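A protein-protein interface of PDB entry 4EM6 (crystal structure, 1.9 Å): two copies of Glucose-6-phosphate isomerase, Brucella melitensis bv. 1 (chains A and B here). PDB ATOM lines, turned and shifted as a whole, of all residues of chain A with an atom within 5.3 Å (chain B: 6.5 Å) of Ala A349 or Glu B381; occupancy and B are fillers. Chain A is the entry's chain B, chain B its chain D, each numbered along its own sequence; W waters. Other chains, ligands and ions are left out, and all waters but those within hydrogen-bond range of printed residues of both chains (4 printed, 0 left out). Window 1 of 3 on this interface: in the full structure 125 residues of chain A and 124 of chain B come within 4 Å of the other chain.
Arg B346 touches its own counterpart, Arg A346.
Printed residues of chain B within 4 Å of Ala A349: Glu B381. Of the printed residues of chain A, Glu B381 touches Arg A346 (3.2 Å) and Ala A349 (3.9 Å). Of the printed residues of chain B, Gln A353 touches Ala B389. Of the printed residues of chain A, Ala B389 touches Gln A353. The nearest residue of chain B that does not touch Ala A349 is Ala B389 (5.2 Å). The nearest printed residue of chain A that does not touch Glu B381 is Gln A352 (4.02 Å).
Of the 18 printed residues of chain B, 5 touch a printed residue of chain A. Printed residues of chain B that touch a printed residue of chain A: Arg B346, Trp B379, Glu B381, Ala B389 and Phe B390. Hydrophobic or aromatic side chains of chain B that line the printed part of chain A: Trp B379 and Phe B390. Hydrophobic or aromatic side chains of chain A that line the printed part of chain B: Ala A349. Along chain A the printed residues that touch a printed residue of chain B span positions 346 to 353. Among the printed residues, 6 pairs touch across the chains. Among the printed residues, Asp or Glu carboxylates within 4 Å of a Lys or Arg side-chain nitrogen of the other chain: Arg A346 with Glu B381 (3.2 Å).
Water W1 lies within hydrogen-bond range of the side-chain carboxylate (OE1) of Glu B381, the backbone carbonyl oxygen (O) of Ser B345 and the guanidinium group (NH1) of Arg A346. Water W2 lies within hydrogen-bond range of the side-chain carboxylate (OE2) of Glu B381 and the side-chain amide oxygen (OE1) of Gln A352. Water W4 lies within hydrogen-bond range of OE2 of Glu B381, NH1 of Arg B346 and NH1 of Arg A346. Water W3 bridges the side-chain amide nitrogen (NE2) of Gln A352 (3.1 Å) and the backbone NH (N) of Gly B380 (3.2 Å).
The backbone carbonyl oxygen (O) of Trp B379 sits at hydrogen-bond distance from the backbone NH (N) of Ile B337, at 2.9 Å.
NH2 of Arg A346 lies within salt-bridge range of OE1 of Glu B381, at 3.2 Å.
Among the printed residues, pairs that only touch across the chains: Arg A346 with Arg B346 (3.5 Å), Ala A349 with Glu B381 (3.9 Å), Gln A352 with Trp B379 (3.7 Å), Gln A352 with Phe B390 (3.6 Å) and Gln A353 with Ala B389 (3.4 Å).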
ATOM      1  N   LEU A 163     -28.769  16.017  17.153  1.00  0.00           N
ATOM      2  CA  LEU A 163     -27.824  16.142  18.240  1.00  0.00           C
ATOM      3  C   LEU A 163     -27.228  14.790  18.623  1.00  0.00           C
ATOM      4  O   LEU A 163     -26.033  14.694  18.892  1.00  0.00           O
ATOM      5  CB  LEU A 163     -28.432  16.829  19.485  1.00  0.00           C
ATOM      6  CG  LEU A 163     -28.840  18.310  19.359  1.00  0.00           C
ATOM      7  CD1 LEU A 163     -29.486  18.788  20.647  1.00  0.00           C
ATOM      8  CD2 LEU A 163     -27.644  19.152  19.055  1.00  0.00           C
ATOM      9  N   ARG A 346     -19.618  17.345  22.169  1.00  0.00           N
ATOM     10  CA  ARG A 346     -21.025  17.640  21.922  1.00  0.00           C
ATOM     11  C   ARG A 346     -22.000  16.821  22.805  1.00  0.00           C
ATOM     12  O   ARG A 346     -23.200  16.777  22.542  1.00  0.00           O
ATOM     13  CB  ARG A 346     -21.325  17.505  20.430  1.00  0.00           C
ATOM     14  CG  ARG A 346     -20.473  18.416  19.536  1.00  0.00           C
ATOM     15  CD  ARG A 346     -20.632  19.894  19.934  1.00  0.00           C
ATOM     16  NE  ARG A 346     -22.004  20.358  19.772  1.00  0.00           N
ATOM     17  CZ  ARG A 346     -22.482  21.516  20.231  1.00  0.00           C
ATOM     18  NH1 ARG A 346     -21.724  22.331  20.939  1.00  0.00           N
ATOM     19  NH2 ARG A 346     -23.727  21.851  19.988  1.00  0.00           N
ATOM     20  N   LEU A 347     -21.487  16.225  23.883  1.00  0.00           N
ATOM     21  CA  LEU A 347     -22.317  15.549  24.876  1.00  0.00           C
ATOM     22  C   LEU A 347     -23.162  16.559  25.674  1.00  0.00           C
ATOM     23  O   LEU A 347     -24.385  16.363  25.804  1.00  0.00           O
ATOM     24  CB  LEU A 347     -21.478  14.667  25.808  1.00  0.00           C
ATOM     25  CG  LEU A 347     -22.250  13.963  26.934  1.00  0.00           C
ATOM     26  CD1 LEU A 347     -23.289  13.004  26.327  1.00  0.00           C
ATOM     27  CD2 LEU A 347     -21.318  13.212  27.918  1.00  0.00           C
ATOM     28  N   PRO A 348     -22.540  17.645  26.196  1.00  0.00           N
ATOM     29  CA  PRO A 348     -23.392  18.595  26.928  1.00  0.00           C
ATOM     30  C   PRO A 348     -24.572  19.113  26.133  1.00  0.00           C
ATOM     31  O   PRO A 348     -25.672  19.162  26.676  1.00  0.00           O
ATOM     32  CB  PRO A 348     -22.416  19.712  27.315  1.00  0.00           C
ATOM     33  CG  PRO A 348     -21.087  18.981  27.430  1.00  0.00           C
ATOM     34  CD  PRO A 348     -21.127  18.065  26.240  1.00  0.00           C
ATOM     35  N   ALA A 349     -24.372  19.444  24.853  1.00  0.00           N
ATOM     36  CA  ALA A 349     -25.443  19.961  24.009  1.00  0.00           C
ATOM     37  C   ALA A 349     -26.518  18.879  23.838  1.00  0.00           C
ATOM     38  O   ALA A 349     -27.739  19.172  23.838  1.00  0.00           O
ATOM     39  CB  ALA A 349     -24.899  20.413  22.636  1.00  0.00           C
ATOM     40  N   TYR A 350     -26.082  17.631  23.686  1.00  0.00           N
ATOM     41  CA  TYR A 350     -27.029  16.509  23.612  1.00  0.00           C
ATOM     42  C   TYR A 350     -27.863  16.365  24.891  1.00  0.00           C
ATOM     43  O   TYR A 350     -29.099  16.198  24.865  1.00  0.00           O
ATOM     44  CB  TYR A 350     -26.282  15.199  23.360  1.00  0.00           C
ATOM     45  CG  TYR A 350     -27.199  13.999  23.297  1.00  0.00           C
ATOM     46  CD1 TYR A 350     -27.795  13.647  22.100  1.00  0.00           C
ATOM     47  CD2 TYR A 350     -27.468  13.216  24.423  1.00  0.00           C
ATOM     48  CE1 TYR A 350     -28.624  12.586  22.001  1.00  0.00           C
ATOM     49  CE2 TYR A 350     -28.331  12.123  24.329  1.00  0.00           C
ATOM     50  CZ  TYR A 350     -28.898  11.812  23.089  1.00  0.00           C
ATOM     51  OH  TYR A 350     -29.734  10.726  22.896  1.00  0.00           O
ATOM     52  N   LEU A 351     -27.170  16.419  26.015  1.00  0.00           N
ATOM     53  CA  LEU A 351     -27.792  16.311  27.308  1.00  0.00           C
ATOM     54  C   LEU A 351     -28.719  17.486  27.613  1.00  0.00           C
ATOM     55  O   LEU A 351     -29.694  17.322  28.351  1.00  0.00           O
ATOM     56  CB  LEU A 351     -26.744  16.135  28.412  1.00  0.00           C
ATOM     57  CG  LEU A 351     -25.879  14.874  28.363  1.00  0.00           C
ATOM     58  CD1 LEU A 351     -24.859  14.942  29.478  1.00  0.00           C
ATOM     59  CD2 LEU A 351     -26.714  13.599  28.446  1.00  0.00           C
ATOM     60  N   GLN A 352     -28.447  18.662  27.049  1.00  0.00           N
ATOM     61  CA  GLN A 352     -29.386  19.783  27.169  1.00  0.00           C
ATOM     62  C   GLN A 352     -30.743  19.445  26.600  1.00  0.00           C
ATOM     63  O   GLN A 352     -31.772  19.753  27.225  1.00  0.00           O
ATOM     64  CB  GLN A 352     -28.905  21.032  26.432  1.00  0.00           C
ATOM     65  CG  GLN A 352     -27.868  21.800  27.146  1.00  0.00           C
ATOM     66  CD  GLN A 352     -27.457  23.064  26.409  1.00  0.00           C
ATOM     67  OE1 GLN A 352     -27.497  23.143  25.156  1.00  0.00           O
ATOM     68  NE2 GLN A 352     -27.053  24.062  27.177  1.00  0.00           N
ATOM     69  N   GLN A 353     -30.774  18.832  25.416  1.00  0.00           N
ATOM     70  CA  GLN A 353     -32.055  18.482  24.850  1.00  0.00           C
ATOM     71  C   GLN A 353     -32.716  17.375  25.682  1.00  0.00           C
ATOM     72  O   GLN A 353     -33.901  17.466  26.023  1.00  0.00           O
ATOM     73  CB  GLN A 353     -32.000  18.101  23.358  1.00  0.00           C
ATOM     74  CG  GLN A 353     -33.419  17.792  22.857  1.00  0.00           C
ATOM     75  CD  GLN A 353     -33.544  17.371  21.396  1.00  0.00           C
ATOM     76  OE1 GLN A 353     -32.555  17.072  20.740  1.00  0.00           O
ATOM     77  NE2 GLN A 353     -34.790  17.367  20.880  1.00  0.00           N
ATOM     78  N   ILE B 337     -27.940  33.213  25.410  1.00  0.00           N
ATOM     79  CA  ILE B 337     -27.530  34.020  24.258  1.00  0.00           C
ATOM     80  C   ILE B 337     -27.661  33.145  23.025  1.00  0.00           C
ATOM     81  O   ILE B 337     -26.937  32.148  22.864  1.00  0.00           O
ATOM     82  CB  ILE B 337     -26.097  34.615  24.423  1.00  0.00           C
ATOM     83  CG1 ILE B 337     -25.986  35.374  25.753  1.00  0.00           C
ATOM     84  CG2 ILE B 337     -25.788  35.579  23.265  1.00  0.00           C
ATOM     85  CD1 ILE B 337     -24.594  36.037  26.010  1.00  0.00           C
ATOM     86  N   ILE B 338     -28.592  33.518  22.146  1.00  0.00           N
ATOM     87  CA  ILE B 338     -29.005  32.661  21.061  1.00  0.00           C
ATOM     88  C   ILE B 338     -28.811  33.417  19.740  1.00  0.00           C
ATOM     89  O   ILE B 338     -29.679  34.204  19.320  1.00  0.00           O
ATOM     90  CB  ILE B 338     -30.457  32.211  21.196  1.00  0.00           C
ATOM     91  CG1 ILE B 338     -30.755  31.657  22.581  1.00  0.00           C
ATOM     92  CG2 ILE B 338     -30.818  31.170  20.112  1.00  0.00           C
ATOM     93  CD1 ILE B 338     -29.940  30.393  22.962  1.00  0.00           C
ATOM     94  N   PRO B 339     -27.654  33.203  19.089  1.00  0.00           N
ATOM     95  CA  PRO B 339     -27.426  33.856  17.821  1.00  0.00           C
ATOM     96  C   PRO B 339     -28.087  33.098  16.686  1.00  0.00           C
ATOM     97  O   PRO B 339     -27.833  31.898  16.509  1.00  0.00           O
ATOM     98  CB  PRO B 339     -25.892  33.849  17.676  1.00  0.00           C
ATOM     99  CG  PRO B 339     -25.428  32.692  18.483  1.00  0.00           C
ATOM    100  CD  PRO B 339     -26.441  32.521  19.595  1.00  0.00           C
ATOM    101  N   TYR B 340     -28.949  33.773  15.928  1.00  0.00           N
ATOM    102  CA  TYR B 340     -29.590  33.160  14.767  1.00  0.00           C
ATOM    103  C   TYR B 340     -28.658  33.214  13.566  1.00  0.00           C
ATOM    104  O   TYR B 340     -28.904  33.927  12.584  1.00  0.00           O
ATOM    105  CB  TYR B 340     -30.966  33.791  14.523  1.00  0.00           C
ATOM    106  CG  TYR B 340     -31.994  33.135  15.415  1.00  0.00           C
ATOM    107  CD1 TYR B 340     -31.936  33.294  16.797  1.00  0.00           C
ATOM    108  CD2 TYR B 340     -32.975  32.307  14.884  1.00  0.00           C
ATOM    109  CE1 TYR B 340     -32.837  32.665  17.636  1.00  0.00           C
ATOM    110  CE2 TYR B 340     -33.906  31.660  15.723  1.00  0.00           C
ATOM    111  CZ  TYR B 340     -33.822  31.847  17.101  1.00  0.00           C
ATOM    112  OH  TYR B 340     -34.708  31.206  17.953  1.00  0.00           O
ATOM    113  N   LEU B 344     -22.125  31.539  13.966  1.00  0.00           N
ATOM    114  CA  LEU B 344     -21.878  31.954  15.350  1.00  0.00           C
ATOM    115  C   LEU B 344     -22.071  30.781  16.338  1.00  0.00           C
ATOM    116  O   LEU B 344     -22.280  30.988  17.526  1.00  0.00           O
ATOM    117  CB  LEU B 344     -22.759  33.154  15.703  1.00  0.00           C
ATOM    118  CG  LEU B 344     -22.461  34.496  14.991  1.00  0.00           C
ATOM    119  CD1 LEU B 344     -23.500  35.607  15.286  1.00  0.00           C
ATOM    120  CD2 LEU B 344     -21.088  34.987  15.390  1.00  0.00           C
ATOM    121  N   SER B 345     -21.908  29.552  15.843  1.00  0.00           N
ATOM    122  CA  SER B 345     -22.031  28.342  16.648  1.00  0.00           C
ATOM    123  C   SER B 345     -21.143  28.351  17.899  1.00  0.00           C
ATOM    124  O   SER B 345     -21.511  27.786  18.922  1.00  0.00           O
ATOM    125  CB  SER B 345     -21.713  27.088  15.824  1.00  0.00           C
ATOM    126  OG  SER B 345     -20.336  27.078  15.410  1.00  0.00           O
ATOM    127  N   ARG B 346     -19.990  28.995  17.840  1.00  0.00           N
ATOM    128  CA  ARG B 346     -19.111  29.008  19.000  1.00  0.00           C
ATOM    129  C   ARG B 346     -19.042  30.361  19.676  1.00  0.00           C
ATOM    130  O   ARG B 346     -18.146  30.605  20.496  1.00  0.00           O
ATOM    131  CB  ARG B 346     -17.738  28.496  18.597  1.00  0.00           C
ATOM    132  CG  ARG B 346     -17.789  27.064  18.002  1.00  0.00           C
ATOM    133  CD  ARG B 346     -18.412  26.045  18.971  1.00  0.00           C
ATOM    134  NE  ARG B 346     -17.650  25.949  20.212  1.00  0.00           N
ATOM    135  CZ  ARG B 346     -18.071  25.353  21.330  1.00  0.00           C
ATOM    136  NH1 ARG B 346     -19.277  24.795  21.417  1.00  0.00           N
ATOM    137  NH2 ARG B 346     -17.288  25.332  22.381  1.00  0.00           N
ATOM    138  N   PRO B 348     -21.595  31.532  21.798  1.00  0.00           N
ATOM    139  CA  PRO B 348     -21.959  31.397  23.217  1.00  0.00           C
ATOM    140  C   PRO B 348     -20.803  30.875  24.092  1.00  0.00           C
ATOM    141  O   PRO B 348     -20.606  31.390  25.201  1.00  0.00           O
ATOM    142  CB  PRO B 348     -23.145  30.426  23.193  1.00  0.00           C
ATOM    143  CG  PRO B 348     -23.729  30.616  21.823  1.00  0.00           C
ATOM    144  CD  PRO B 348     -22.554  30.842  20.924  1.00  0.00           C
ATOM    145  N   TRP B 379     -25.042  30.844  28.648  1.00  0.00           N
ATOM    146  CA  TRP B 379     -25.101  29.637  27.869  1.00  0.00           C
ATOM    147  C   TRP B 379     -25.918  29.908  26.614  1.00  0.00           C
ATOM    148  O   TRP B 379     -26.564  30.934  26.499  1.00  0.00           O
ATOM    149  CB  TRP B 379     -25.717  28.502  28.710  1.00  0.00           C
ATOM    150  CG  TRP B 379     -27.128  28.766  29.186  1.00  0.00           C
ATOM    151  CD1 TRP B 379     -27.526  29.535  30.246  1.00  0.00           C
ATOM    152  CD2 TRP B 379     -28.317  28.223  28.617  1.00  0.00           C
ATOM    153  NE1 TRP B 379     -28.897  29.496  30.363  1.00  0.00           N
ATOM    154  CE2 TRP B 379     -29.401  28.705  29.366  1.00  0.00           C
ATOM    155  CE3 TRP B 379     -28.570  27.383  27.518  1.00  0.00           C
ATOM    156  CZ2 TRP B 379     -30.733  28.370  29.066  1.00  0.00           C
ATOM    157  CZ3 TRP B 379     -29.909  27.049  27.212  1.00  0.00           C
ATOM    158  CH2 TRP B 379     -30.966  27.557  27.972  1.00  0.00           C
ATOM    159  N   GLY B 380     -25.835  29.005  25.652  1.00  0.00           N
ATOM    160  CA  GLY B 380     -26.643  29.093  24.456  1.00  0.00           C
ATOM    161  C   GLY B 380     -26.111  28.218  23.333  1.00  0.00           C
ATOM    162  O   GLY B 380     -25.037  27.579  23.446  1.00  0.00           O
ATOM    163  N   GLU B 381     -26.921  28.160  22.283  1.00  0.00           N
ATOM    164  CA  GLU B 381     -26.581  27.559  21.013  1.00  0.00           C
ATOM    165  C   GLU B 381     -27.210  28.454  19.955  1.00  0.00           C
ATOM    166  O   GLU B 381     -28.132  29.252  20.267  1.00  0.00           O
ATOM    167  CB  GLU B 381     -27.172  26.147  20.897  1.00  0.00           C
ATOM    168  CG  GLU B 381     -26.490  25.063  21.775  1.00  0.00           C
ATOM    169  CD  GLU B 381     -25.099  24.670  21.292  1.00  0.00           C
ATOM    170  OE1 GLU B 381     -24.812  24.847  20.108  1.00  0.00           O
ATOM    171  OE2 GLU B 381     -24.272  24.191  22.116  1.00  0.00           O
ATOM    172  N   PRO B 382     -26.768  28.324  18.694  1.00  0.00           N
ATOM    173  CA  PRO B 382     -27.418  29.099  17.647  1.00  0.00           C
ATOM    174  C   PRO B 382     -28.891  28.750  17.436  1.00  0.00           C
ATOM    175  O   PRO B 382     -29.319  27.609  17.697  1.00  0.00           O
ATOM    176  CB  PRO B 382     -26.618  28.748  16.387  1.00  0.00           C
ATOM    177  CG  PRO B 382     -25.893  27.502  16.704  1.00  0.00           C
ATOM    178  CD  PRO B 382     -25.670  27.486  18.172  1.00  0.00           C
ATOM    179  N   GLY B 383     -29.667  29.738  17.007  1.00  0.00           N
ATOM    180  CA  GLY B 383     -31.010  29.496  16.445  1.00  0.00           C
ATOM    181  C   GLY B 383     -30.822  29.143  14.966  1.00  0.00           C
ATOM    182  O   GLY B 383     -29.896  29.657  14.352  1.00  0.00           O
ATOM    183  N   ASN B 385     -31.355  25.947  15.776  1.00  0.00           N
ATOM    184  CA  ASN B 385     -30.973  24.694  16.464  1.00  0.00           C
ATOM    185  C   ASN B 385     -31.474  24.656  17.923  1.00  0.00           C
ATOM    186  O   ASN B 385     -32.090  23.681  18.361  1.00  0.00           O
ATOM    187  CB  ASN B 385     -29.455  24.469  16.490  1.00  0.00           C
ATOM    188  CG  ASN B 385     -28.772  24.648  15.131  1.00  0.00           C
ATOM    189  OD1 ASN B 385     -29.415  24.960  14.132  1.00  0.00           O
ATOM    190  ND2 ASN B 385     -27.440  24.452  15.108  1.00  0.00           N
ATOM    191  N   GLY B 386     -31.193  25.710  18.672  1.00  0.00           N
ATOM    192  CA  GLY B 386     -31.582  25.767  20.082  1.00  0.00           C
ATOM    193  C   GLY B 386     -33.068  25.618  20.349  1.00  0.00           C
ATOM    194  O   GLY B 386     -33.453  25.056  21.373  1.00  0.00           O
ATOM    195  N   ALA B 389     -33.911  22.138  20.837  1.00  0.00           N
ATOM    196  CA  ALA B 389     -33.157  21.493  21.868  1.00  0.00           C
ATOM    197  C   ALA B 389     -33.753  21.855  23.219  1.00  0.00           C
ATOM    198  O   ALA B 389     -34.113  20.976  23.969  1.00  0.00           O
ATOM    199  CB  ALA B 389     -31.684  21.921  21.812  1.00  0.00           C
ATOM    200  N   PHE B 390     -33.821  23.145  23.534  1.00  0.00           N
ATOM    201  CA  PHE B 390     -34.134  23.562  24.894  1.00  0.00           C
ATOM    202  C   PHE B 390     -35.145  24.678  25.053  1.00  0.00           C
ATOM    203  O   PHE B 390     -35.392  25.077  26.174  1.00  0.00           O
ATOM    204  CB  PHE B 390     -32.869  23.947  25.646  1.00  0.00           C
ATOM    205  CG  PHE B 390     -31.978  24.901  24.890  1.00  0.00           C
ATOM    206  CD1 PHE B 390     -32.317  26.235  24.759  1.00  0.00           C
ATOM    207  CD2 PHE B 390     -30.796  24.452  24.308  1.00  0.00           C
ATOM    208  CE1 PHE B 390     -31.517  27.115  24.077  1.00  0.00           C
ATOM    209  CE2 PHE B 390     -29.978  25.337  23.613  1.00  0.00           C
ATOM    210  CZ  PHE B 390     -30.324  26.677  23.514  1.00  0.00           C
ATOM    211  N   PHE B 391     -35.714  25.202  23.966  1.00  0.00           N
ATOM    212  CA  PHE B 391     -36.683  26.289  24.126  1.00  0.00           C
ATOM    213  C   PHE B 391     -37.977  25.833  24.832  1.00  0.00           C
ATOM    214  O   PHE B 391     -38.688  26.655  25.397  1.00  0.00           O
ATOM    215  CB  PHE B 391     -37.002  26.957  22.796  1.00  0.00           C
ATOM    216  CG  PHE B 391     -36.106  28.130  22.475  1.00  0.00           C
ATOM    217  CD1 PHE B 391     -34.749  27.960  22.311  1.00  0.00           C
ATOM    218  CD2 PHE B 391     -36.631  29.423  22.382  1.00  0.00           C
ATOM    219  CE1 PHE B 391     -33.928  29.039  22.004  1.00  0.00           C
ATOM    220  CE2 PHE B 391     -35.808  30.502  22.086  1.00  0.00           C
ATOM    221  CZ  PHE B 391     -34.465  30.304  21.898  1.00  0.00           C
HETATM  222  O   HOH W   1     -22.434  25.123  19.137  1.00  0.00           O
HETATM  223  O   HOH W   2     -24.952  23.942  24.599  1.00  0.00           O
HETATM  224  O   HOH W   3     -24.896  26.027  26.288  1.00  0.00           O
HETATM  225  O   HOH W   4     -21.556  24.295  23.214  1.00  0.00           O
